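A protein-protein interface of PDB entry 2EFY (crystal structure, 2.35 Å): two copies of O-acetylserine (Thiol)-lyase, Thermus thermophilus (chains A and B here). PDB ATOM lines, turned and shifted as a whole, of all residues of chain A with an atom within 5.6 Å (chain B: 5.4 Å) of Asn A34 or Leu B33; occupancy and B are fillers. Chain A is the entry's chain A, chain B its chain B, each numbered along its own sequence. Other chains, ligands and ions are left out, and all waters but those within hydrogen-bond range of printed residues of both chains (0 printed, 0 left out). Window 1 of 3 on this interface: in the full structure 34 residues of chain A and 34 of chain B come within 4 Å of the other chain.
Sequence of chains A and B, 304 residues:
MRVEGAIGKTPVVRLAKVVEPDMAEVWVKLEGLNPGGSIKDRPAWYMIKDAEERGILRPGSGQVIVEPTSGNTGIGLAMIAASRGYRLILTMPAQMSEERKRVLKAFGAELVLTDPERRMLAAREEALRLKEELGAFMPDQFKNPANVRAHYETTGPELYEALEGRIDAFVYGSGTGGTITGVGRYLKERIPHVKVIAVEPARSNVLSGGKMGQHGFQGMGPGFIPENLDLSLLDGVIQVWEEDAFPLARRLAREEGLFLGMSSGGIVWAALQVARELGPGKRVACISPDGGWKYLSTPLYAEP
Of the printed residues of chain B, Leu A33 touches Leu B33 (3.9 Å), Asn B34 (3.7 Å) and Pro B35 (3.9 Å).
Asn A34 touches just one residue of chain B: Leu B33.
Of the printed residues of chain A, Pro B11 touches Ala A6 (3.7 Å).
Leu B33 touches just these residues of chain A: Leu A33 (3.9 Å), Asn A34 (3.6 Å) and Pro A35 (3.7 Å).
The nearest printed residue of chain B that does not touch Asn A34 is Gly B32 (6.6 Å).
The nearest residue of chain A that does not touch Leu B33 is Ala A6 (4.8 Å).
The nearest printed residue of chain B that does not touch Leu A33 is Gly B32 (6.0 Å).
The backbone NH (N) of Gly A8 is in hydrogen-bond range of the side-chain amide oxygen (OD1) of Asn A34 (2.7 Å).
O of Glu A31 sits at hydrogen-bond distance from ND2 of Asn A34, at 2.9 Å.
The backbone carbonyl oxygen of Ser A38 lies within hydrogen-bond range of the side-chain amide nitrogen of Asn A34, 3.4 Å away.
The backbone carbonyl oxygen of Pro B11 is in hydrogen-bond range of the backbone NH of Leu B30 (2.9 Å).
The side-chain carboxylate (OE2) of Glu B31 lies within hydrogen-bond range of the side-chain amide nitrogen (ND2) of Asn B34 (3.0 Å).
Of the 17 printed residues of chain A, 4 touch a printed residue of chain B.
Of the 9 printed residues of chain B, 4 touch a printed residue of chain A.
Printed residues of chain B that touch a printed residue of chain A: Pro B11, Leu B33, Asn B34 and Pro B35.
Hydrophobic or aromatic side chains of chain B within 4 Å of the printed part of chain A: Pro B11 and Leu B33.
Among the printed residues, 6 pairs touch across the chains.
Pro B11 touches Ala A6 (CG to CB, 3.7 Å).
Leu A33 touches Leu B33.
Asn B34 touches Leu A33 (O to CD2, 3.7 Å).
CA of Pro B35 touches CD2 of Leu A33 (3.9 Å).
Asn A34 touches Leu B33.
Pro A35 touches Leu B33.
Leu B33 touches its own counterpart, Leu A33.
Leu A33 touches Asn B34, and with the chains exchanged Asn A34 touches Leu B33.
Leu A33 touches Pro B35, and with the chains exchanged Pro A35 touches Leu B33.
8 positions are printed for both chains.
Of the 6 pairs that touch across the chains among the printed residues, 5 have their exchanged pair printed and touching as well.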
ATOM      1  N   ALA A   6       6.880   1.780  16.875  1.00  0.00           N
ATOM      2  CA  ALA A   6       6.535   1.786  18.299  1.00  0.00           C
ATOM      3  C   ALA A   6       5.253   1.011  18.610  1.00  0.00           C
ATOM      4  O   ALA A   6       4.800   0.974  19.758  1.00  0.00           O
ATOM      5  CB  ALA A   6       6.400   3.234  18.798  1.00  0.00           C
ATOM      6  N   ILE A   7       4.673   0.400  17.583  1.00  0.00           N
ATOM      7  CA  ILE A   7       3.449  -0.372  17.731  1.00  0.00           C
ATOM      8  C   ILE A   7       3.735  -1.752  18.326  1.00  0.00           C
ATOM      9  O   ILE A   7       4.699  -2.421  17.940  1.00  0.00           O
ATOM     10  CB  ILE A   7       2.737  -0.542  16.350  1.00  0.00           C
ATOM     11  CG1 ILE A   7       2.189   0.815  15.875  1.00  0.00           C
ATOM     12  CG2 ILE A   7       1.629  -1.588  16.447  1.00  0.00           C
ATOM     13  CD1 ILE A   7       1.630   0.822  14.449  1.00  0.00           C
ATOM     14  N   GLY A   8       2.895  -2.167  19.272  1.00  0.00           N
ATOM     15  CA  GLY A   8       3.054  -3.470  19.890  1.00  0.00           C
ATOM     16  C   GLY A   8       3.907  -3.490  21.139  1.00  0.00           C
ATOM     17  O   GLY A   8       4.174  -2.443  21.740  1.00  0.00           O
ATOM     18  N   LYS A   9       4.339  -4.693  21.519  1.00  0.00           N
ATOM     19  CA  LYS A   9       5.168  -4.905  22.706  1.00  0.00           C
ATOM     20  C   LYS A   9       4.450  -4.361  23.939  1.00  0.00           C
ATOM     21  O   LYS A   9       5.066  -3.805  24.847  1.00  0.00           O
ATOM     22  CB  LYS A   9       6.528  -4.214  22.548  1.00  0.00           C
ATOM     23  CG  LYS A   9       7.344  -4.673  21.340  1.00  0.00           C
ATOM     24  CD  LYS A   9       7.731  -6.140  21.440  1.00  0.00           C
ATOM     25  CE  LYS A   9       8.518  -6.587  20.212  1.00  0.00           C
ATOM     26  NZ  LYS A   9       7.739  -6.397  18.947  1.00  0.00           N
ATOM     27  N   THR A  10       3.136  -4.532  23.964  1.00  0.00           N
ATOM     28  CA  THR A  10       2.337  -4.052  25.077  1.00  0.00           C
ATOM     29  C   THR A  10       2.483  -4.959  26.286  1.00  0.00           C
ATOM     30  O   THR A  10       2.738  -6.158  26.158  1.00  0.00           O
ATOM     31  CB  THR A  10       0.870  -3.964  24.678  1.00  0.00           C
ATOM     32  OG1 THR A  10       0.459  -5.216  24.118  1.00  0.00           O
ATOM     33  CG2 THR A  10       0.673  -2.848  23.645  1.00  0.00           C
ATOM     34  N   LEU A  30      -2.629  -5.009  27.649  1.00  0.00           N
ATOM     35  CA  LEU A  30      -3.113  -3.634  27.480  1.00  0.00           C
ATOM     36  C   LEU A  30      -2.774  -2.999  26.125  1.00  0.00           C
ATOM     37  O   LEU A  30      -1.764  -2.290  25.991  1.00  0.00           O
ATOM     38  CB  LEU A  30      -2.571  -2.761  28.627  1.00  0.00           C
ATOM     39  CG  LEU A  30      -2.773  -3.343  30.046  1.00  0.00           C
ATOM     40  CD1 LEU A  30      -2.143  -2.443  31.120  1.00  0.00           C
ATOM     41  CD2 LEU A  30      -4.256  -3.521  30.317  1.00  0.00           C
ATOM     42  N   GLU A  31      -3.628  -3.246  25.130  1.00  0.00           N
ATOM     43  CA  GLU A  31      -3.426  -2.705  23.790  1.00  0.00           C
ATOM     44  C   GLU A  31      -3.715  -1.210  23.736  1.00  0.00           C
ATOM     45  O   GLU A  31      -3.463  -0.553  22.720  1.00  0.00           O
ATOM     46  CB  GLU A  31      -4.306  -3.430  22.768  1.00  0.00           C
ATOM     47  CG  GLU A  31      -3.800  -4.818  22.374  1.00  0.00           C
ATOM     48  CD  GLU A  31      -2.348  -4.809  21.901  1.00  0.00           C
ATOM     49  OE1 GLU A  31      -1.452  -5.160  22.695  1.00  0.00           O
ATOM     50  OE2 GLU A  31      -2.103  -4.441  20.737  1.00  0.00           O
ATOM     51  N   GLY A  32      -4.247  -0.674  24.826  1.00  0.00           N
ATOM     52  CA  GLY A  32      -4.527   0.746  24.858  1.00  0.00           C
ATOM     53  C   GLY A  32      -3.211   1.499  24.919  1.00  0.00           C
ATOM     54  O   GLY A  32      -3.173   2.707  24.729  1.00  0.00           O
ATOM     55  N   LEU A  33      -2.119   0.779  25.173  1.00  0.00           N
ATOM     56  CA  LEU A  33      -0.811   1.420  25.269  1.00  0.00           C
ATOM     57  C   LEU A  33      -0.034   1.516  23.949  1.00  0.00           C
ATOM     58  O   LEU A  33       1.181   1.707  23.939  1.00  0.00           O
ATOM     59  CB  LEU A  33       0.039   0.726  26.342  1.00  0.00           C
ATOM     60  CG  LEU A  33      -0.617   0.610  27.732  1.00  0.00           C
ATOM     61  CD1 LEU A  33       0.418   0.135  28.741  1.00  0.00           C
ATOM     62  CD2 LEU A  33      -1.203   1.954  28.174  1.00  0.00           C
ATOM     63  N   ASN A  34      -0.736   1.373  22.834  1.00  0.00           N
ATOM     64  CA  ASN A  34      -0.104   1.499  21.527  1.00  0.00           C
ATOM     65  C   ASN A  34      -0.065   2.993  21.177  1.00  0.00           C
ATOM     66  O   ASN A  34      -0.837   3.788  21.717  1.00  0.00           O
ATOM     67  CB  ASN A  34      -0.907   0.735  20.470  1.00  0.00           C
ATOM     68  CG  ASN A  34      -0.580  -0.745  20.444  1.00  0.00           C
ATOM     69  OD1 ASN A  34       0.542  -1.136  20.112  1.00  0.00           O
ATOM     70  ND2 ASN A  34      -1.553  -1.576  20.797  1.00  0.00           N
ATOM     71  N   PRO A  35       0.835   3.396  20.269  1.00  0.00           N
ATOM     72  CA  PRO A  35       0.955   4.804  19.864  1.00  0.00           C
ATOM     73  C   PRO A  35      -0.379   5.481  19.531  1.00  0.00           C
ATOM     74  O   PRO A  35      -0.597   6.645  19.865  1.00  0.00           O
ATOM     75  CB  PRO A  35       1.888   4.730  18.656  1.00  0.00           C
ATOM     76  CG  PRO A  35       2.804   3.598  19.037  1.00  0.00           C
ATOM     77  CD  PRO A  35       1.837   2.560  19.582  1.00  0.00           C
ATOM     78  N   GLY A  36      -1.265   4.745  18.872  1.00  0.00           N
ATOM     79  CA  GLY A  36      -2.561   5.292  18.506  1.00  0.00           C
ATOM     80  C   GLY A  36      -3.649   5.060  19.545  1.00  0.00           C
ATOM     81  O   GLY A  36      -4.826   5.302  19.283  1.00  0.00           O
ATOM     82  N   GLY A  37      -3.263   4.567  20.719  1.00  0.00           N
ATOM     83  CA  GLY A  37      -4.226   4.346  21.787  1.00  0.00           C
ATOM     84  C   GLY A  37      -5.076   3.089  21.728  1.00  0.00           C
ATOM     85  O   GLY A  37      -5.926   2.894  22.592  1.00  0.00           O
ATOM     86  N   SER A  38      -4.883   2.235  20.728  1.00  0.00           N
ATOM     87  CA  SER A  38      -5.679   1.014  20.672  1.00  0.00           C
ATOM     88  C   SER A  38      -5.020  -0.101  19.886  1.00  0.00           C
ATOM     89  O   SER A  38      -4.031   0.096  19.187  1.00  0.00           O
ATOM     90  CB  SER A  38      -7.061   1.281  20.064  1.00  0.00           C
ATOM     91  OG  SER A  38      -7.027   1.124  18.652  1.00  0.00           O
ATOM     92  N   ILE A  39      -5.605  -1.279  20.009  1.00  0.00           N
ATOM     93  CA  ILE A  39      -5.124  -2.466  19.331  1.00  0.00           C
ATOM     94  C   ILE A  39      -5.170  -2.303  17.798  1.00  0.00           C
ATOM     95  O   ILE A  39      -4.490  -3.029  17.068  1.00  0.00           O
ATOM     96  CB  ILE A  39      -5.987  -3.660  19.734  1.00  0.00           C
ATOM     97  CG1 ILE A  39      -5.391  -4.958  19.187  1.00  0.00           C
ATOM     98  CG2 ILE A  39      -7.412  -3.455  19.217  1.00  0.00           C
ATOM     99  CD1 ILE A  39      -6.102  -6.190  19.672  1.00  0.00           C
ATOM    100  N   ASP A  41      -3.830  -0.173  15.958  1.00  0.00           N
ATOM    101  CA  ASP A  41      -2.552   0.272  15.400  1.00  0.00           C
ATOM    102  C   ASP A  41      -1.987  -0.880  14.567  1.00  0.00           C
ATOM    103  O   ASP A  41      -1.552  -0.688  13.429  1.00  0.00           O
ATOM    104  CB  ASP A  41      -1.550   0.598  16.520  1.00  0.00           C
ATOM    105  CG  ASP A  41      -1.731   1.990  17.099  1.00  0.00           C
ATOM    106  OD1 ASP A  41      -2.817   2.590  16.936  1.00  0.00           O
ATOM    107  OD2 ASP A  41      -0.774   2.484  17.735  1.00  0.00           O
ATOM    108  N   ARG A  42      -2.004  -2.079  15.146  1.00  0.00           N
ATOM    109  CA  ARG A  42      -1.479  -3.269  14.487  1.00  0.00           C
ATOM    110  C   ARG A  42      -2.118  -3.523  13.119  1.00  0.00           C
ATOM    111  O   ARG A  42      -1.428  -3.524  12.105  1.00  0.00           O
ATOM    112  CB  ARG A  42      -1.652  -4.487  15.400  1.00  0.00           C
ATOM    113  CG  ARG A  42      -1.015  -4.339  16.781  1.00  0.00           C
ATOM    114  CD  ARG A  42      -1.170  -5.623  17.571  1.00  0.00           C
ATOM    115  NE  ARG A  42      -0.756  -5.507  18.966  1.00  0.00           N
ATOM    116  CZ  ARG A  42       0.475  -5.729  19.415  1.00  0.00           C
ATOM    117  NH1 ARG A  42       1.445  -6.081  18.573  1.00  0.00           N
ATOM    118  NH2 ARG A  42       0.729  -5.626  20.713  1.00  0.00           N
ATOM    119  N   THR B  10       9.068   2.757  27.663  1.00  0.00           N
ATOM    120  CA  THR B  10       8.430   3.449  26.562  1.00  0.00           C
ATOM    121  C   THR B  10       9.381   3.554  25.374  1.00  0.00           C
ATOM    122  O   THR B  10      10.597   3.624  25.542  1.00  0.00           O
ATOM    123  CB  THR B  10       7.992   4.851  27.002  1.00  0.00           C
ATOM    124  OG1 THR B  10       9.147   5.620  27.371  1.00  0.00           O
ATOM    125  CG2 THR B  10       7.039   4.748  28.205  1.00  0.00           C
ATOM    126  N   PRO B  11       8.831   3.561  24.154  1.00  0.00           N
ATOM    127  CA  PRO B  11       9.611   3.655  22.915  1.00  0.00           C
ATOM    128  C   PRO B  11      10.136   5.061  22.636  1.00  0.00           C
ATOM    129  O   PRO B  11       9.664   6.040  23.219  1.00  0.00           O
ATOM    130  CB  PRO B  11       8.614   3.209  21.857  1.00  0.00           C
ATOM    131  CG  PRO B  11       7.325   3.788  22.383  1.00  0.00           C
ATOM    132  CD  PRO B  11       7.392   3.442  23.861  1.00  0.00           C
ATOM    133  N   LEU B  30       8.413   8.569  23.946  1.00  0.00           N
ATOM    134  CA  LEU B  30       6.984   8.776  24.165  1.00  0.00           C
ATOM    135  C   LEU B  30       6.428   8.327  25.513  1.00  0.00           C
ATOM    136  O   LEU B  30       5.969   7.195  25.655  1.00  0.00           O
ATOM    137  CB  LEU B  30       6.197   8.092  23.051  1.00  0.00           C
ATOM    138  CG  LEU B  30       6.672   8.399  21.632  1.00  0.00           C
ATOM    139  CD1 LEU B  30       5.897   7.534  20.647  1.00  0.00           C
ATOM    140  CD2 LEU B  30       6.485   9.888  21.330  1.00  0.00           C
ATOM    141  N   GLU B  31       6.437   9.232  26.487  1.00  0.00           N
ATOM    142  CA  GLU B  31       5.938   8.922  27.817  1.00  0.00           C
ATOM    143  C   GLU B  31       4.407   8.862  27.888  1.00  0.00           C
ATOM    144  O   GLU B  31       3.835   8.475  28.914  1.00  0.00           O
ATOM    145  CB  GLU B  31       6.476   9.944  28.819  1.00  0.00           C
ATOM    146  CG  GLU B  31       7.962   9.760  29.149  1.00  0.00           C
ATOM    147  CD  GLU B  31       8.253   8.398  29.759  1.00  0.00           C
ATOM    148  OE1 GLU B  31       8.834   7.534  29.066  1.00  0.00           O
ATOM    149  OE2 GLU B  31       7.886   8.188  30.934  1.00  0.00           O
ATOM    150  N   GLY B  32       3.745   9.227  26.792  1.00  0.00           N
ATOM    151  CA  GLY B  32       2.294   9.200  26.762  1.00  0.00           C
ATOM    152  C   GLY B  32       1.806   7.768  26.709  1.00  0.00           C
ATOM    153  O   GLY B  32       0.637   7.491  26.969  1.00  0.00           O
ATOM    154  N   LEU B  33       2.713   6.852  26.383  1.00  0.00           N
ATOM    155  CA  LEU B  33       2.368   5.439  26.293  1.00  0.00           C
ATOM    156  C   LEU B  33       2.469   4.652  27.616  1.00  0.00           C
ATOM    157  O   LEU B  33       2.529   3.426  27.604  1.00  0.00           O
ATOM    158  CB  LEU B  33       3.219   4.768  25.215  1.00  0.00           C
ATOM    159  CG  LEU B  33       3.168   5.444  23.841  1.00  0.00           C
ATOM    160  CD1 LEU B  33       3.889   4.571  22.816  1.00  0.00           C
ATOM    161  CD2 LEU B  33       1.712   5.670  23.417  1.00  0.00           C
ATOM    162  N   ASN B  34       2.502   5.353  28.743  1.00  0.00           N
ATOM    163  CA  ASN B  34       2.530   4.712  30.059  1.00  0.00           C
ATOM    164  C   ASN B  34       1.070   4.402  30.437  1.00  0.00           C
ATOM    165  O   ASN B  34       0.140   4.997  29.892  1.00  0.00           O
ATOM    166  CB  ASN B  34       3.125   5.657  31.110  1.00  0.00           C
ATOM    167  CG  ASN B  34       4.635   5.589  31.177  1.00  0.00           C
ATOM    168  OD1 ASN B  34       5.201   4.538  31.465  1.00  0.00           O
ATOM    169  ND2 ASN B  34       5.297   6.709  30.920  1.00  0.00           N
ATOM    170  N   PRO B  35       0.852   3.474  31.384  1.00  0.00           N
ATOM    171  CA  PRO B  35      -0.506   3.109  31.814  1.00  0.00           C
ATOM    172  C   PRO B  35      -1.422   4.300  32.108  1.00  0.00           C
ATOM    173  O   PRO B  35      -2.566   4.334  31.656  1.00  0.00           O
ATOM    174  CB  PRO B  35      -0.254   2.264  33.058  1.00  0.00           C
ATOM    175  CG  PRO B  35       1.027   1.559  32.717  1.00  0.00           C
ATOM    176  CD  PRO B  35       1.865   2.672  32.100  1.00  0.00           C
ATOM    177  N   GLY B  37      -1.075   7.235  31.018  1.00  0.00           N
ATOM    178  CA  GLY B  37      -1.058   8.185  29.921  1.00  0.00           C
ATOM    179  C   GLY B  37      -0.002   9.275  29.938  1.00  0.00           C
ATOM    180  O   GLY B  37       0.011  10.107  29.032  1.00  0.00           O
